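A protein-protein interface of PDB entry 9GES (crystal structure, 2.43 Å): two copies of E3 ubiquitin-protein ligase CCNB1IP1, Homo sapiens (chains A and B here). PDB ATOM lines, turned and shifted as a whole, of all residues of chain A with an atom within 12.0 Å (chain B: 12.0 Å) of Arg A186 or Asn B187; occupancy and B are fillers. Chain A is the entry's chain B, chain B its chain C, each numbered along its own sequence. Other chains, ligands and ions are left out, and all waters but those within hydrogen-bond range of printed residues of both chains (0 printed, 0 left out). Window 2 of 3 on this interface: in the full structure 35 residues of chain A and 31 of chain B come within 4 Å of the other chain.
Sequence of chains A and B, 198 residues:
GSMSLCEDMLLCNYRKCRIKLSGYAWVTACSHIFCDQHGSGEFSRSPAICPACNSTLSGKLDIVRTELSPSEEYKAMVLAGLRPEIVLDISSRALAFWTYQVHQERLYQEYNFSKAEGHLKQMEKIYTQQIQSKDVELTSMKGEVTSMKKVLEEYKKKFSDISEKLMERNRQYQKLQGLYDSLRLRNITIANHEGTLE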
ATOM      1  N   LEU A 176      -9.723  24.327  -1.473  1.00  0.00           N
ATOM      2  CA  LEU A 176      -8.459  23.940  -2.088  1.00  0.00           C
ATOM      3  C   LEU A 176      -7.292  24.135  -1.128  1.00  0.00           C
ATOM      4  O   LEU A 176      -6.298  23.404  -1.204  1.00  0.00           O
ATOM      5  CB  LEU A 176      -8.238  24.735  -3.375  1.00  0.00           C
ATOM      6  CG  LEU A 176      -7.077  24.297  -4.270  1.00  0.00           C
ATOM      7  CD1 LEU A 176      -7.182  22.816  -4.584  1.00  0.00           C
ATOM      8  CD2 LEU A 176      -7.053  25.113  -5.552  1.00  0.00           C
ATOM      9  N   GLN A 177      -7.389  25.117  -0.228  1.00  0.00           N
ATOM     10  CA  GLN A 177      -6.375  25.277   0.810  1.00  0.00           C
ATOM     11  C   GLN A 177      -6.325  24.055   1.719  1.00  0.00           C
ATOM     12  O   GLN A 177      -5.239  23.588   2.087  1.00  0.00           O
ATOM     13  CB  GLN A 177      -6.654  26.543   1.621  1.00  0.00           C
ATOM     14  CG  GLN A 177      -5.775  26.710   2.845  1.00  0.00           C
ATOM     15  CD  GLN A 177      -6.214  27.868   3.719  1.00  0.00           C
ATOM     16  OE1 GLN A 177      -7.089  28.648   3.343  1.00  0.00           O
ATOM     17  NE2 GLN A 177      -5.610  27.981   4.895  1.00  0.00           N
ATOM     18  N   GLY A 178      -7.492  23.526   2.095  1.00  0.00           N
ATOM     19  CA  GLY A 178      -7.522  22.319   2.907  1.00  0.00           C
ATOM     20  C   GLY A 178      -6.952  21.114   2.184  1.00  0.00           C
ATOM     21  O   GLY A 178      -6.235  20.303   2.778  1.00  0.00           O
ATOM     22  N   LEU A 179      -7.270  20.973   0.894  1.00  0.00           N
ATOM     23  CA  LEU A 179      -6.694  19.889   0.103  1.00  0.00           C
ATOM     24  C   LEU A 179      -5.184  20.047  -0.030  1.00  0.00           C
ATOM     25  O   LEU A 179      -4.442  19.058   0.011  1.00  0.00           O
ATOM     26  CB  LEU A 179      -7.353  19.837  -1.276  1.00  0.00           C
ATOM     27  CG  LEU A 179      -8.865  19.607  -1.291  1.00  0.00           C
ATOM     28  CD1 LEU A 179      -9.391  19.542  -2.716  1.00  0.00           C
ATOM     29  CD2 LEU A 179      -9.224  18.344  -0.525  1.00  0.00           C
ATOM     30  N   TYR A 180      -4.711  21.284  -0.201  1.00  0.00           N
ATOM     31  CA  TYR A 180      -3.273  21.524  -0.261  1.00  0.00           C
ATOM     32  C   TYR A 180      -2.596  21.158   1.054  1.00  0.00           C
ATOM     33  O   TYR A 180      -1.499  20.587   1.058  1.00  0.00           O
ATOM     34  CB  TYR A 180      -2.996  22.984  -0.621  1.00  0.00           C
ATOM     35  CG  TYR A 180      -1.559  23.398  -0.404  1.00  0.00           C
ATOM     36  CD1 TYR A 180      -0.548  22.933  -1.238  1.00  0.00           C
ATOM     37  CD2 TYR A 180      -1.210  24.254   0.632  1.00  0.00           C
ATOM     38  CE1 TYR A 180       0.767  23.305  -1.045  1.00  0.00           C
ATOM     39  CE2 TYR A 180       0.102  24.633   0.833  1.00  0.00           C
ATOM     40  CZ  TYR A 180       1.088  24.156  -0.008  1.00  0.00           C
ATOM     41  OH  TYR A 180       2.395  24.533   0.194  1.00  0.00           O
ATOM     42  N   ASP A 181      -3.232  21.486   2.182  1.00  0.00           N
ATOM     43  CA  ASP A 181      -2.677  21.118   3.482  1.00  0.00           C
ATOM     44  C   ASP A 181      -2.618  19.603   3.645  1.00  0.00           C
ATOM     45  O   ASP A 181      -1.649  19.068   4.196  1.00  0.00           O
ATOM     46  CB  ASP A 181      -3.504  21.755   4.600  1.00  0.00           C
ATOM     47  CG  ASP A 181      -2.798  21.728   5.945  1.00  0.00           C
ATOM     48  OD1 ASP A 181      -1.671  21.194   6.026  1.00  0.00           O
ATOM     49  OD2 ASP A 181      -3.371  22.248   6.925  1.00  0.00           O
ATOM     50  N   SER A 182      -3.651  18.896   3.177  1.00  0.00           N
ATOM     51  CA  SER A 182      -3.641  17.438   3.247  1.00  0.00           C
ATOM     52  C   SER A 182      -2.494  16.853   2.431  1.00  0.00           C
ATOM     53  O   SER A 182      -1.813  15.923   2.879  1.00  0.00           O
ATOM     54  CB  SER A 182      -4.981  16.882   2.768  1.00  0.00           C
ATOM     55  OG  SER A 182      -4.977  15.466   2.788  1.00  0.00           O
ATOM     56  N   LEU A 183      -2.268  17.380   1.225  1.00  0.00           N
ATOM     57  CA  LEU A 183      -1.126  16.940   0.432  1.00  0.00           C
ATOM     58  C   LEU A 183       0.191  17.463   0.988  1.00  0.00           C
ATOM     59  O   LEU A 183       1.247  16.907   0.671  1.00  0.00           O
ATOM     60  CB  LEU A 183      -1.285  17.375  -1.026  1.00  0.00           C
ATOM     61  CG  LEU A 183      -2.307  16.619  -1.875  1.00  0.00           C
ATOM     62  CD1 LEU A 183      -2.005  16.816  -3.353  1.00  0.00           C
ATOM     63  CD2 LEU A 183      -2.330  15.139  -1.522  1.00  0.00           C
ATOM     64  N   ARG A 184       0.155  18.527   1.791  1.00  0.00           N
ATOM     65  CA  ARG A 184       1.366  18.966   2.476  1.00  0.00           C
ATOM     66  C   ARG A 184       1.814  17.940   3.509  1.00  0.00           C
ATOM     67  O   ARG A 184       3.017  17.727   3.700  1.00  0.00           O
ATOM     68  CB  ARG A 184       1.143  20.325   3.136  1.00  0.00           C
ATOM     69  CG  ARG A 184       2.389  20.903   3.783  1.00  0.00           C
ATOM     70  CD  ARG A 184       2.033  21.920   4.849  1.00  0.00           C
ATOM     71  NE  ARG A 184       1.275  23.040   4.304  1.00  0.00           N
ATOM     72  CZ  ARG A 184       0.673  23.959   5.045  1.00  0.00           C
ATOM     73  NH1 ARG A 184       0.704  23.913   6.366  1.00  0.00           N
ATOM     74  NH2 ARG A 184       0.019  24.950   4.443  1.00  0.00           N
ATOM     75  N   LEU A 185       0.857  17.293   4.182  1.00  0.00           N
ATOM     76  CA  LEU A 185       1.192  16.217   5.107  1.00  0.00           C
ATOM     77  C   LEU A 185       1.872  15.056   4.396  1.00  0.00           C
ATOM     78  O   LEU A 185       2.620  14.300   5.024  1.00  0.00           O
ATOM     79  CB  LEU A 185      -0.067  15.727   5.825  1.00  0.00           C
ATOM     80  CG  LEU A 185      -0.662  16.635   6.901  1.00  0.00           C
ATOM     81  CD1 LEU A 185      -1.959  16.048   7.430  1.00  0.00           C
ATOM     82  CD2 LEU A 185       0.330  16.846   8.032  1.00  0.00           C
ATOM     83  N   ARG A 186       1.612  14.889   3.103  1.00  0.00           N
ATOM     84  CA  ARG A 186       2.240  13.838   2.310  1.00  0.00           C
ATOM     85  C   ARG A 186       3.741  14.054   2.201  1.00  0.00           C
ATOM     86  O   ARG A 186       4.514  13.447   2.937  1.00  0.00           O
ATOM     87  CB  ARG A 186       1.619  13.780   0.918  1.00  0.00           C
ATOM     88  CG  ARG A 186       2.240  12.761  -0.017  1.00  0.00           C
ATOM     89  CD  ARG A 186       1.822  13.057  -1.451  1.00  0.00           C
ATOM     90  NE  ARG A 186       2.491  14.240  -1.981  1.00  0.00           N
ATOM     91  CZ  ARG A 186       2.182  14.834  -3.127  1.00  0.00           C
ATOM     92  NH1 ARG A 186       1.193  14.396  -3.890  1.00  0.00           N
ATOM     93  NH2 ARG A 186       2.885  15.892  -3.519  1.00  0.00           N
ATOM     94  N   LEU B 176      -3.120  28.348  -7.203  1.00  0.00           N
ATOM     95  CA  LEU B 176      -3.188  27.238  -6.257  1.00  0.00           C
ATOM     96  C   LEU B 176      -3.606  25.943  -6.943  1.00  0.00           C
ATOM     97  O   LEU B 176      -3.159  24.860  -6.547  1.00  0.00           O
ATOM     98  CB  LEU B 176      -4.153  27.576  -5.116  1.00  0.00           C
ATOM     99  CG  LEU B 176      -4.145  26.629  -3.911  1.00  0.00           C
ATOM    100  CD1 LEU B 176      -2.735  26.476  -3.369  1.00  0.00           C
ATOM    101  CD2 LEU B 176      -5.089  27.137  -2.829  1.00  0.00           C
ATOM    102  N   GLN B 177      -4.470  26.031  -7.958  1.00  0.00           N
ATOM    103  CA  GLN B 177      -4.801  24.851  -8.751  1.00  0.00           C
ATOM    104  C   GLN B 177      -3.565  24.287  -9.443  1.00  0.00           C
ATOM    105  O   GLN B 177      -3.341  23.071  -9.444  1.00  0.00           O
ATOM    106  CB  GLN B 177      -5.875  25.189  -9.785  1.00  0.00           C
ATOM    107  CG  GLN B 177      -7.289  25.253  -9.247  1.00  0.00           C
ATOM    108  CD  GLN B 177      -8.313  25.446 -10.351  1.00  0.00           C
ATOM    109  OE1 GLN B 177      -7.962  25.716 -11.501  1.00  0.00           O
ATOM    110  NE2 GLN B 177      -9.587  25.302 -10.006  1.00  0.00           N
ATOM    111  N   GLY B 178      -2.755  25.159 -10.045  1.00  0.00           N
ATOM    112  CA  GLY B 178      -1.548  24.691 -10.705  1.00  0.00           C
ATOM    113  C   GLY B 178      -0.556  24.071  -9.741  1.00  0.00           C
ATOM    114  O   GLY B 178       0.067  23.050 -10.043  1.00  0.00           O
ATOM    115  N   LEU B 179      -0.386  24.686  -8.567  1.00  0.00           N
ATOM    116  CA  LEU B 179       0.501  24.114  -7.560  1.00  0.00           C
ATOM    117  C   LEU B 179      -0.014  22.765  -7.080  1.00  0.00           C
ATOM    118  O   LEU B 179       0.768  21.826  -6.885  1.00  0.00           O
ATOM    119  CB  LEU B 179       0.656  25.078  -6.385  1.00  0.00           C
ATOM    120  CG  LEU B 179       1.221  26.460  -6.722  1.00  0.00           C
ATOM    121  CD1 LEU B 179       1.335  27.317  -5.471  1.00  0.00           C
ATOM    122  CD2 LEU B 179       2.565  26.339  -7.422  1.00  0.00           C
ATOM    123  N   TYR B 180      -1.329  22.649  -6.880  1.00  0.00           N
ATOM    124  CA  TYR B 180      -1.910  21.376  -6.463  1.00  0.00           C
ATOM    125  C   TYR B 180      -1.720  20.306  -7.532  1.00  0.00           C
ATOM    126  O   TYR B 180      -1.415  19.150  -7.214  1.00  0.00           O
ATOM    127  CB  TYR B 180      -3.394  21.560  -6.142  1.00  0.00           C
ATOM    128  CG  TYR B 180      -4.076  20.313  -5.625  1.00  0.00           C
ATOM    129  CD1 TYR B 180      -4.677  19.413  -6.497  1.00  0.00           C
ATOM    130  CD2 TYR B 180      -4.125  20.039  -4.266  1.00  0.00           C
ATOM    131  CE1 TYR B 180      -5.302  18.273  -6.031  1.00  0.00           C
ATOM    132  CE2 TYR B 180      -4.750  18.903  -3.789  1.00  0.00           C
ATOM    133  CZ  TYR B 180      -5.335  18.022  -4.676  1.00  0.00           C
ATOM    134  OH  TYR B 180      -5.957  16.888  -4.206  1.00  0.00           O
ATOM    135  N   ASP B 181      -1.909  20.668  -8.804  1.00  0.00           N
ATOM    136  CA  ASP B 181      -1.752  19.698  -9.883  1.00  0.00           C
ATOM    137  C   ASP B 181      -0.311  19.215  -9.992  1.00  0.00           C
ATOM    138  O   ASP B 181      -0.062  18.017 -10.183  1.00  0.00           O
ATOM    139  CB  ASP B 181      -2.223  20.303 -11.206  1.00  0.00           C
ATOM    140  CG  ASP B 181      -3.714  20.589 -11.215  1.00  0.00           C
ATOM    141  OD1 ASP B 181      -4.461  19.871 -10.517  1.00  0.00           O
ATOM    142  OD2 ASP B 181      -4.140  21.529 -11.922  1.00  0.00           O
ATOM    143  N   SER B 182       0.654  20.131  -9.882  1.00  0.00           N
ATOM    144  CA  SER B 182       2.055  19.726  -9.856  1.00  0.00           C
ATOM    145  C   SER B 182       2.359  18.896  -8.616  1.00  0.00           C
ATOM    146  O   SER B 182       3.149  17.946  -8.670  1.00  0.00           O
ATOM    147  CB  SER B 182       2.960  20.956  -9.911  1.00  0.00           C
ATOM    148  OG  SER B 182       2.807  21.754  -8.749  1.00  0.00           O
ATOM    149  N   LEU B 183       1.746  19.250  -7.485  1.00  0.00           N
ATOM    150  CA  LEU B 183       1.913  18.467  -6.266  1.00  0.00           C
ATOM    151  C   LEU B 183       1.371  17.055  -6.445  1.00  0.00           C
ATOM    152  O   LEU B 183       1.981  16.083  -5.984  1.00  0.00           O
ATOM    153  CB  LEU B 183       1.213  19.174  -5.108  1.00  0.00           C
ATOM    154  CG  LEU B 183       1.651  18.894  -3.673  1.00  0.00           C
ATOM    155  CD1 LEU B 183       3.137  19.178  -3.507  1.00  0.00           C
ATOM    156  CD2 LEU B 183       0.828  19.734  -2.705  1.00  0.00           C
ATOM    157  N   ARG B 184       0.224  16.922  -7.119  1.00  0.00           N
ATOM    158  CA  ARG B 184      -0.330  15.603  -7.403  1.00  0.00           C
ATOM    159  C   ARG B 184       0.566  14.818  -8.354  1.00  0.00           C
ATOM    160  O   ARG B 184       0.755  13.608  -8.181  1.00  0.00           O
ATOM    161  CB  ARG B 184      -1.734  15.746  -7.988  1.00  0.00           C
ATOM    162  CG  ARG B 184      -2.419  14.426  -8.297  1.00  0.00           C
ATOM    163  CD  ARG B 184      -3.537  14.616  -9.304  1.00  0.00           C
ATOM    164  NE  ARG B 184      -4.519  15.598  -8.860  1.00  0.00           N
ATOM    165  CZ  ARG B 184      -5.469  16.104  -9.633  1.00  0.00           C
ATOM    166  NH1 ARG B 184      -5.588  15.751 -10.902  1.00  0.00           N
ATOM    167  NH2 ARG B 184      -6.321  16.988  -9.120  1.00  0.00           N
ATOM    168  N   LEU B 185       1.126  15.493  -9.364  1.00  0.00           N
ATOM    169  CA  LEU B 185       2.012  14.823 -10.313  1.00  0.00           C
ATOM    170  C   LEU B 185       3.262  14.283  -9.634  1.00  0.00           C
ATOM    171  O   LEU B 185       3.825  13.277 -10.081  1.00  0.00           O
ATOM    172  CB  LEU B 185       2.403  15.782 -11.440  1.00  0.00           C
ATOM    173  CG  LEU B 185       1.391  15.991 -12.564  1.00  0.00           C
ATOM    174  CD1 LEU B 185       1.898  17.030 -13.548  1.00  0.00           C
ATOM    175  CD2 LEU B 185       1.117  14.675 -13.271  1.00  0.00           C
ATOM    176  N   ARG B 186       3.718  14.946  -8.568  1.00  0.00           N
ATOM    177  CA  ARG B 186       4.901  14.481  -7.852  1.00  0.00           C
ATOM    178  C   ARG B 186       4.678  13.093  -7.260  1.00  0.00           C
ATOM    179  O   ARG B 186       5.579  12.248  -7.286  1.00  0.00           O
ATOM    180  CB  ARG B 186       5.273  15.484  -6.759  1.00  0.00           C
ATOM    181  CG  ARG B 186       6.504  15.113  -5.945  1.00  0.00           C
ATOM    182  CD  ARG B 186       7.751  15.045  -6.806  1.00  0.00           C
ATOM    183  NE  ARG B 186       8.958  14.878  -6.005  1.00  0.00           N
ATOM    184  CZ  ARG B 186      10.162  14.646  -6.510  1.00  0.00           C
ATOM    185  NH1 ARG B 186      10.352  14.528  -7.814  1.00  0.00           N
ATOM    186  NH2 ARG B 186      11.200  14.525  -5.686  1.00  0.00           N
ATOM    187  N   ASN B 187       3.489  12.843  -6.720  1.00  0.00           N
ATOM    188  CA  ASN B 187       3.168  11.541  -6.144  1.00  0.00           C
ATOM    189  C   ASN B 187       1.948  10.924  -6.821  1.00  0.00           C
ATOM    190  O   ASN B 187       1.864   9.705  -6.984  1.00  0.00           O
ATOM    191  CB  ASN B 187       2.932  11.668  -4.639  1.00  0.00           C
ATOM    192  CG  ASN B 187       4.141  12.217  -3.909  1.00  0.00           C
ATOM    193  OD1 ASN B 187       4.554  13.351  -4.142  1.00  0.00           O
ATOM    194  ND2 ASN B 187       4.715  11.415  -3.020  1.00  0.00           N
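O of Leu B183 lies within hydrogen-bond range of NH2 of Arg A186. The guanidinium group (NH2) of Arg A186 sits close to the side-chain amide oxygen (OD1) of Asn B187, 3.1 Å away.
Leu B176 touches Leu A176. Gln B177 touches Leu A176. CB of Leu A179 touches CE2 of Tyr B180, at 3.7 Å. Tyr A180 touches Leu B183 (CD1 to CD2, 3.8 Å). Tyr B180 touches Leu A183 (CE2 to CD1, 3.5 Å). Leu A183 touches Leu B183.
Printed residues of chain B within 4 Å of Arg A186: Leu B183 (2.6 Å) and Asn B187 (3.0 Å). Of chain A, only Arg A186 comes within 4 Å of Asn B187. No residue of chain B comes within 4 Å of Ser A182. Printed residues of chain B within 4 Å of Leu A183: Tyr B180 (3.5 Å) and Leu B183 (3.6 Å). Of the printed residues of chain A, Leu B183 touches Tyr A180, Leu A183 and Arg A186. No residue of chain A comes within 4 Å of Arg B186. Printed residues of chain A within 4 Å of Leu B176: Leu A176 (3.7 Å). Of the printed residues of chain B, Tyr A180 touches Leu B183. Printed residues of chain A within 4 Å of Gln B177: Leu A176 (3.6 Å). The nearest printed residue of chain B that does not touch Arg A186 is Arg B184 (4.01 Å). The nearest residue of chain A that does not touch Asn B187 is Leu A183 (6.8 Å). The nearest printed residue of chain B that does not touch Leu A176 is Tyr B180 (4.1 Å).
Hydrophobic or aromatic side chains of chain A that line the printed part of chain B: Leu A176, Leu A179, Tyr A180 and Leu A183. Hydrophobic or aromatic side chains of chain B that line the printed part of chain A: Leu B176, Tyr B180 and Leu B183. Along chain B the printed residues that touch a printed residue of chain A span positions 176 to 187. Among the printed residues, no Asp or Glu carboxylate lies within 4 Å of a Lys or Arg side-chain nitrogen of the other chain.
Leu B176 touches its own counterpart, Leu A176. Leu A176 touches Gln B177, but with the chains exchanged Gln A177 does not touch Leu B176 (4.02 Å). Leu A179 touches Tyr B180, but with the chains exchanged Tyr A180 does not touch Leu B179 (5.6 Å). Tyr A180 touches Leu B183, and with the chains exchanged Leu A183 touches Tyr B180. 11 positions are printed for both chains.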
